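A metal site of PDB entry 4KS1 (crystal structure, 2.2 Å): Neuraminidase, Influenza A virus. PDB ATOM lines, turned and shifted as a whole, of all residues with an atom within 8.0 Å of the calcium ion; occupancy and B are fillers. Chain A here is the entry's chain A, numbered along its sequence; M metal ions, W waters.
The backbone carbonyl oxygen (O) of Tyr 264 lies close to the side-chain amide oxygen (OD1) of Asn 213. OD2 of Asp 212 lies within hydrogen-bond range of N of Trp 214 (2.8 Å). The backbone NH (N) of Thr 215 is in hydrogen-bond range of the side-chain carboxylate (OD2) of Asp 212 (3.0 Å). The side-chain carboxylate (OD1) of Asp 212 is in hydrogen-bond range of the side-chain hydroxyl (OH) of Tyr 234. The side-chain carboxylate of Asp 242 is in salt-bridge range of the guanidinium group of Arg 219. O of Asp 242 lies within hydrogen-bond range of NH2 of Arg 245, at 3.2 Å. The side-chain amide oxygen (OD1) of Asn 213 lies within hydrogen-bond range of the backbone NH (N) of Gly 265 (3.1 Å). The backbone carbonyl oxygen (O) of Gly 265 is in hydrogen-bond range of the guanidinium group (NH1) of Arg 211.
Residues that only touch the calcium ion: Gly 265. Of the 25 residues printed, 5 come within 4 Å of the calcium ion.
The calcium ion is bound by O of Tyr 264 (2.3 Å), O of Asp 212 (2.3 Å), O of Gly 216 (2.4 Å), OD1 of Asp 242 (2.4 Å), water W2 (2.5 Å) and water W1 (2.6 Å). The calcium ion has six donor atoms within binding distance.
Water W2 lies within hydrogen-bond range of the backbone carbonyl oxygen (O) of Gly 263 (2.7 Å) and the backbone carbonyl oxygen (O) of Pro 244 (2.8 Å).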
ATOM      1  N   HIS A 193     -18.509  20.995  24.065  1.00  0.00           N
ATOM      2  CA  HIS A 193     -17.716  21.479  25.176  1.00  0.00           C
ATOM      3  C   HIS A 193     -17.417  22.966  24.965  1.00  0.00           C
ATOM      4  O   HIS A 193     -16.947  23.370  23.899  1.00  0.00           O
ATOM      5  CB  HIS A 193     -16.418  20.681  25.259  1.00  0.00           C
ATOM      6  CG  HIS A 193     -15.708  20.810  26.578  1.00  0.00           C
ATOM      7  ND1 HIS A 193     -14.597  21.605  26.748  1.00  0.00           N
ATOM      8  CD2 HIS A 193     -15.930  20.208  27.766  1.00  0.00           C
ATOM      9  CE1 HIS A 193     -14.169  21.504  28.002  1.00  0.00           C
ATOM     10  NE2 HIS A 193     -14.973  20.663  28.639  1.00  0.00           N
ATOM     11  N   CYS A 210     -15.787  30.072  20.953  1.00  0.00           N
ATOM     12  CA  CYS A 210     -15.185  29.544  22.176  1.00  0.00           C
ATOM     13  C   CYS A 210     -14.182  28.436  21.947  1.00  0.00           C
ATOM     14  O   CYS A 210     -13.684  28.257  20.836  1.00  0.00           O
ATOM     15  CB  CYS A 210     -16.275  29.069  23.138  1.00  0.00           C
ATOM     16  SG  CYS A 210     -17.645  30.224  23.225  1.00  0.00           S
ATOM     17  N   ARG A 211     -13.897  27.695  23.014  1.00  0.00           N
ATOM     18  CA  ARG A 211     -12.896  26.632  22.974  1.00  0.00           C
ATOM     19  C   ARG A 211     -13.530  25.308  23.385  1.00  0.00           C
ATOM     20  O   ARG A 211     -14.051  25.188  24.486  1.00  0.00           O
ATOM     21  CB  ARG A 211     -11.730  26.977  23.904  1.00  0.00           C
ATOM     22  CG  ARG A 211     -10.780  25.823  24.260  1.00  0.00           C
ATOM     23  CD  ARG A 211      -9.731  26.289  25.282  1.00  0.00           C
ATOM     24  NE  ARG A 211      -8.839  25.210  25.701  1.00  0.00           N
ATOM     25  CZ  ARG A 211      -7.789  25.366  26.518  1.00  0.00           C
ATOM     26  NH1 ARG A 211      -7.036  24.328  26.848  1.00  0.00           N
ATOM     27  NH2 ARG A 211      -7.486  26.571  27.011  1.00  0.00           N
ATOM     28  N   ASP A 212     -13.499  24.329  22.480  1.00  0.00           N
ATOM     29  CA  ASP A 212     -13.858  22.967  22.820  1.00  0.00           C
ATOM     30  C   ASP A 212     -12.580  22.271  23.278  1.00  0.00           C
ATOM     31  O   ASP A 212     -11.667  22.055  22.496  1.00  0.00           O
ATOM     32  CB  ASP A 212     -14.461  22.248  21.602  1.00  0.00           C
ATOM     33  CG  ASP A 212     -14.910  20.813  21.907  1.00  0.00           C
ATOM     34  OD1 ASP A 212     -16.054  20.464  21.570  1.00  0.00           O
ATOM     35  OD2 ASP A 212     -14.116  20.025  22.464  1.00  0.00           O
ATOM     36  N   ASN A 213     -12.524  21.920  24.565  1.00  0.00           N
ATOM     37  CA  ASN A 213     -11.356  21.266  25.128  1.00  0.00           C
ATOM     38  C   ASN A 213     -11.554  19.747  25.264  1.00  0.00           C
ATOM     39  O   ASN A 213     -10.742  19.060  25.884  1.00  0.00           O
ATOM     40  CB  ASN A 213     -10.990  21.892  26.480  1.00  0.00           C
ATOM     41  CG  ASN A 213      -9.512  21.753  26.815  1.00  0.00           C
ATOM     42  OD1 ASN A 213      -8.653  22.271  26.103  1.00  0.00           O
ATOM     43  ND2 ASN A 213      -9.220  21.049  27.909  1.00  0.00           N
ATOM     44  N   TRP A 214     -12.627  19.240  24.669  1.00  0.00           N
ATOM     45  CA  TRP A 214     -13.020  17.833  24.747  1.00  0.00           C
ATOM     46  C   TRP A 214     -12.593  17.013  23.517  1.00  0.00           C
ATOM     47  O   TRP A 214     -11.642  16.234  23.590  1.00  0.00           O
ATOM     48  CB  TRP A 214     -14.541  17.728  24.962  1.00  0.00           C
ATOM     49  CG  TRP A 214     -15.064  16.345  25.264  1.00  0.00           C
ATOM     50  CD1 TRP A 214     -14.334  15.211  25.430  1.00  0.00           C
ATOM     51  CD2 TRP A 214     -16.442  15.970  25.448  1.00  0.00           C
ATOM     52  NE1 TRP A 214     -15.164  14.143  25.697  1.00  0.00           N
ATOM     53  CE2 TRP A 214     -16.464  14.591  25.711  1.00  0.00           C
ATOM     54  CE3 TRP A 214     -17.652  16.673  25.407  1.00  0.00           C
ATOM     55  CZ2 TRP A 214     -17.649  13.890  25.927  1.00  0.00           C
ATOM     56  CZ3 TRP A 214     -18.823  15.978  25.629  1.00  0.00           C
ATOM     57  CH2 TRP A 214     -18.818  14.598  25.878  1.00  0.00           C
ATOM     58  N   THR A 215     -13.301  17.181  22.409  1.00  0.00           N
ATOM     59  CA  THR A 215     -12.990  16.428  21.197  1.00  0.00           C
ATOM     60  C   THR A 215     -12.799  17.299  19.939  1.00  0.00           C
ATOM     61  O   THR A 215     -12.251  16.837  18.946  1.00  0.00           O
ATOM     62  CB  THR A 215     -14.080  15.382  20.860  1.00  0.00           C
ATOM     63  OG1 THR A 215     -15.243  16.057  20.342  1.00  0.00           O
ATOM     64  CG2 THR A 215     -14.457  14.552  22.089  1.00  0.00           C
ATOM     65  N   GLY A 216     -13.251  18.548  19.998  1.00  0.00           N
ATOM     66  CA  GLY A 216     -13.333  19.385  18.809  1.00  0.00           C
ATOM     67  C   GLY A 216     -12.107  20.216  18.488  1.00  0.00           C
ATOM     68  O   GLY A 216     -11.478  20.799  19.377  1.00  0.00           O
ATOM     69  N   THR A 217     -11.756  20.266  17.196  1.00  0.00           N
ATOM     70  CA  THR A 217     -10.695  21.160  16.736  1.00  0.00           C
ATOM     71  C   THR A 217     -11.308  22.346  15.985  1.00  0.00           C
ATOM     72  O   THR A 217     -10.602  23.255  15.549  1.00  0.00           O
ATOM     73  CB  THR A 217      -9.673  20.436  15.855  1.00  0.00           C
ATOM     74  OG1 THR A 217     -10.319  20.004  14.638  1.00  0.00           O
ATOM     75  CG2 THR A 217      -9.091  19.234  16.583  1.00  0.00           C
ATOM     76  N   ASN A 218     -12.633  22.301  15.822  1.00  0.00           N
ATOM     77  CA  ASN A 218     -13.376  23.486  15.427  1.00  0.00           C
ATOM     78  C   ASN A 218     -13.928  24.160  16.691  1.00  0.00           C
ATOM     79  O   ASN A 218     -13.961  23.538  17.745  1.00  0.00           O
ATOM     80  CB  ASN A 218     -14.503  23.152  14.445  1.00  0.00           C
ATOM     81  CG  ASN A 218     -15.415  22.030  14.932  1.00  0.00           C
ATOM     82  OD1 ASN A 218     -15.125  21.351  15.917  1.00  0.00           O
ATOM     83  ND2 ASN A 218     -16.532  21.839  14.237  1.00  0.00           N
ATOM     84  N   ARG A 219     -14.309  25.423  16.592  1.00  0.00           N
ATOM     85  CA  ARG A 219     -14.716  26.186  17.768  1.00  0.00           C
ATOM     86  C   ARG A 219     -16.223  26.281  17.949  1.00  0.00           C
ATOM     87  O   ARG A 219     -16.951  26.568  16.989  1.00  0.00           O
ATOM     88  CB  ARG A 219     -14.090  27.591  17.729  1.00  0.00           C
ATOM     89  CG  ARG A 219     -12.576  27.573  17.809  1.00  0.00           C
ATOM     90  CD  ARG A 219     -11.989  28.930  18.114  1.00  0.00           C
ATOM     91  NE  ARG A 219     -10.525  28.875  18.206  1.00  0.00           N
ATOM     92  CZ  ARG A 219      -9.856  28.593  19.324  1.00  0.00           C
ATOM     93  NH1 ARG A 219      -8.538  28.564  19.312  1.00  0.00           N
ATOM     94  NH2 ARG A 219     -10.519  28.334  20.448  1.00  0.00           N
ATOM     95  N   PRO A 220     -16.703  26.052  19.181  1.00  0.00           N
ATOM     96  CA  PRO A 220     -18.108  26.255  19.533  1.00  0.00           C
ATOM     97  C   PRO A 220     -18.530  27.693  19.276  1.00  0.00           C
ATOM     98  O   PRO A 220     -17.714  28.595  19.467  1.00  0.00           O
ATOM     99  CB  PRO A 220     -18.146  25.981  21.040  1.00  0.00           C
ATOM    100  CG  PRO A 220     -16.967  25.118  21.297  1.00  0.00           C
ATOM    101  CD  PRO A 220     -15.915  25.533  20.322  1.00  0.00           C
ATOM    102  N   TYR A 234     -21.269  24.946  16.332  1.00  0.00           N
ATOM    103  CA  TYR A 234     -19.872  25.120  15.969  1.00  0.00           C
ATOM    104  C   TYR A 234     -19.727  26.051  14.790  1.00  0.00           C
ATOM    105  O   TYR A 234     -20.631  26.150  13.943  1.00  0.00           O
ATOM    106  CB  TYR A 234     -19.188  23.770  15.708  1.00  0.00           C
ATOM    107  CG  TYR A 234     -18.920  23.020  16.990  1.00  0.00           C
ATOM    108  CD1 TYR A 234     -19.939  22.311  17.628  1.00  0.00           C
ATOM    109  CD2 TYR A 234     -17.668  23.063  17.591  1.00  0.00           C
ATOM    110  CE1 TYR A 234     -19.709  21.645  18.812  1.00  0.00           C
ATOM    111  CE2 TYR A 234     -17.429  22.396  18.785  1.00  0.00           C
ATOM    112  CZ  TYR A 234     -18.462  21.693  19.390  1.00  0.00           C
ATOM    113  OH  TYR A 234     -18.241  21.032  20.572  1.00  0.00           O
ATOM    114  N   SER A 241      -9.775  25.817  13.633  1.00  0.00           N
ATOM    115  CA  SER A 241      -9.019  26.951  14.158  1.00  0.00           C
ATOM    116  C   SER A 241      -8.611  26.799  15.624  1.00  0.00           C
ATOM    117  O   SER A 241      -8.194  27.773  16.270  1.00  0.00           O
ATOM    118  CB  SER A 241      -9.780  28.262  13.930  1.00  0.00           C
ATOM    119  OG  SER A 241     -10.904  28.378  14.792  1.00  0.00           O
ATOM    120  N   ASP A 242      -8.694  25.577  16.155  1.00  0.00           N
ATOM    121  CA  ASP A 242      -8.223  25.329  17.523  1.00  0.00           C
ATOM    122  C   ASP A 242      -6.782  24.815  17.477  1.00  0.00           C
ATOM    123  O   ASP A 242      -6.234  24.592  16.401  1.00  0.00           O
ATOM    124  CB  ASP A 242      -9.159  24.339  18.230  1.00  0.00           C
ATOM    125  CG  ASP A 242      -9.043  24.384  19.766  1.00  0.00           C
ATOM    126  OD1 ASP A 242      -9.801  23.635  20.412  1.00  0.00           O
ATOM    127  OD2 ASP A 242      -8.219  25.148  20.323  1.00  0.00           O
ATOM    128  N   THR A 243      -6.159  24.660  18.645  1.00  0.00           N
ATOM    129  CA  THR A 243      -4.807  24.110  18.713  1.00  0.00           C
ATOM    130  C   THR A 243      -4.666  23.247  19.961  1.00  0.00           C
ATOM    131  O   THR A 243      -4.812  23.748  21.076  1.00  0.00           O
ATOM    132  CB  THR A 243      -3.741  25.225  18.737  1.00  0.00           C
ATOM    133  OG1 THR A 243      -3.948  26.135  17.641  1.00  0.00           O
ATOM    134  CG2 THR A 243      -2.341  24.630  18.632  1.00  0.00           C
ATOM    135  N   PRO A 244      -4.331  21.954  19.782  1.00  0.00           N
ATOM    136  CA  PRO A 244      -3.905  21.315  18.539  1.00  0.00           C
ATOM    137  C   PRO A 244      -5.055  21.025  17.584  1.00  0.00           C
ATOM    138  O   PRO A 244      -6.212  20.919  17.998  1.00  0.00           O
ATOM    139  CB  PRO A 244      -3.327  19.990  19.025  1.00  0.00           C
ATOM    140  CG  PRO A 244      -4.181  19.648  20.186  1.00  0.00           C
ATOM    141  CD  PRO A 244      -4.456  20.978  20.880  1.00  0.00           C
ATOM    142  N   ARG A 245      -4.723  20.880  16.302  1.00  0.00           N
ATOM    143  CA  ARG A 245      -5.705  20.590  15.272  1.00  0.00           C
ATOM    144  C   ARG A 245      -5.050  19.765  14.172  1.00  0.00           C
ATOM    145  O   ARG A 245      -3.830  19.602  14.153  1.00  0.00           O
ATOM    146  CB  ARG A 245      -6.242  21.897  14.679  1.00  0.00           C
ATOM    147  CG  ARG A 245      -5.261  22.604  13.751  1.00  0.00           C
ATOM    148  CD  ARG A 245      -5.815  23.921  13.232  1.00  0.00           C
ATOM    149  NE  ARG A 245      -4.786  24.687  12.535  1.00  0.00           N
ATOM    150  CZ  ARG A 245      -3.958  25.557  13.122  1.00  0.00           C
ATOM    151  NH1 ARG A 245      -3.052  26.201  12.405  1.00  0.00           N
ATOM    152  NH2 ARG A 245      -4.041  25.777  14.429  1.00  0.00           N
ATOM    153  N   MET A 259     -15.639  18.489  15.458  1.00  0.00           N
ATOM    154  CA  MET A 259     -14.913  17.661  14.503  1.00  0.00           C
ATOM    155  C   MET A 259     -13.418  17.675  14.824  1.00  0.00           C
ATOM    156  O   MET A 259     -12.924  18.588  15.487  1.00  0.00           O
ATOM    157  CB  MET A 259     -15.143  18.174  13.078  1.00  0.00           C
ATOM    158  CG  MET A 259     -16.581  18.060  12.597  1.00  0.00           C
ATOM    159  SD  MET A 259     -16.959  16.415  11.931  1.00  0.00           S
ATOM    160  CE  MET A 259     -17.629  16.912  10.346  1.00  0.00           C
ATOM    161  N   ASN A 261     -11.630  15.116  16.341  1.00  0.00           N
ATOM    162  CA  ASN A 261     -11.303  14.084  17.321  1.00  0.00           C
ATOM    163  C   ASN A 261      -9.931  14.258  18.005  1.00  0.00           C
ATOM    164  O   ASN A 261      -9.107  13.358  18.002  1.00  0.00           O
ATOM    165  CB  ASN A 261     -11.396  12.698  16.674  1.00  0.00           C
ATOM    166  CG  ASN A 261     -11.501  11.583  17.688  1.00  0.00           C
ATOM    167  OD1 ASN A 261     -12.213  11.703  18.696  1.00  0.00           O
ATOM    168  ND2 ASN A 261     -10.780  10.501  17.448  1.00  0.00           N
ATOM    169  N   GLN A 262      -9.692  15.440  18.570  1.00  0.00           N
ATOM    170  CA  GLN A 262      -8.482  15.683  19.340  1.00  0.00           C
ATOM    171  C   GLN A 262      -8.830  16.401  20.638  1.00  0.00           C
ATOM    172  O   GLN A 262      -9.769  17.190  20.680  1.00  0.00           O
ATOM    173  CB  GLN A 262      -7.481  16.532  18.556  1.00  0.00           C
ATOM    174  CG  GLN A 262      -6.835  15.823  17.383  1.00  0.00           C
ATOM    175  CD  GLN A 262      -5.676  16.598  16.810  1.00  0.00           C
ATOM    176  OE1 GLN A 262      -5.712  17.033  15.659  1.00  0.00           O
ATOM    177  NE2 GLN A 262      -4.623  16.754  17.604  1.00  0.00           N
ATOM    178  N   GLY A 263      -8.059  16.128  21.685  1.00  0.00           N
ATOM    179  CA  GLY A 263      -8.264  16.783  22.961  1.00  0.00           C
ATOM    180  C   GLY A 263      -7.559  18.134  23.035  1.00  0.00           C
ATOM    181  O   GLY A 263      -6.998  18.603  22.040  1.00  0.00           O
ATOM    182  N   TYR A 264      -7.616  18.750  24.211  1.00  0.00           N
ATOM    183  CA  TYR A 264      -6.986  20.051  24.469  1.00  0.00           C
ATOM    184  C   TYR A 264      -7.529  21.156  23.559  1.00  0.00           C
ATOM    185  O   TYR A 264      -8.549  20.991  22.896  1.00  0.00           O
ATOM    186  CB  TYR A 264      -5.452  19.948  24.387  1.00  0.00           C
ATOM    187  CG  TYR A 264      -4.701  20.971  25.235  1.00  0.00           C
ATOM    188  CD1 TYR A 264      -5.108  21.263  26.538  1.00  0.00           C
ATOM    189  CD2 TYR A 264      -3.571  21.610  24.745  1.00  0.00           C
ATOM    190  CE1 TYR A 264      -4.403  22.181  27.327  1.00  0.00           C
ATOM    191  CE2 TYR A 264      -2.871  22.532  25.511  1.00  0.00           C
ATOM    192  CZ  TYR A 264      -3.286  22.810  26.800  1.00  0.00           C
ATOM    193  OH  TYR A 264      -2.578  23.723  27.558  1.00  0.00           O
ATOM    194  N   GLY A 265      -6.821  22.284  23.543  1.00  0.00           N
ATOM    195  CA  GLY A 265      -7.249  23.442  22.793  1.00  0.00           C
ATOM    196  C   GLY A 265      -6.513  24.690  23.227  1.00  0.00           C
ATOM    197  O   GLY A 265      -5.524  24.620  23.963  1.00  0.00           O
ATOM    198  N   VAL A 266      -6.980  25.841  22.770  1.00  0.00           N
ATOM    199  CA  VAL A 266      -6.422  27.120  23.167  1.00  0.00           C
ATOM    200  C   VAL A 266      -7.525  28.157  22.990  1.00  0.00           C
ATOM    201  O   VAL A 266      -8.352  28.009  22.088  1.00  0.00           O
ATOM    202  CB  VAL A 266      -5.159  27.471  22.338  1.00  0.00           C
ATOM    203  CG1 VAL A 266      -5.513  27.709  20.883  1.00  0.00           C
ATOM    204  CG2 VAL A 266      -4.409  28.667  22.924  1.00  0.00           C
HETATM  205 CA    CA M   1      -9.960  21.360  21.136  1.00  0.00          CA
HETATM  206  O   HOH W   1     -10.477  19.010  22.067  1.00  0.00           O
HETATM  207  O   HOH W   2      -7.883  20.403  20.231  1.00  0.00           O
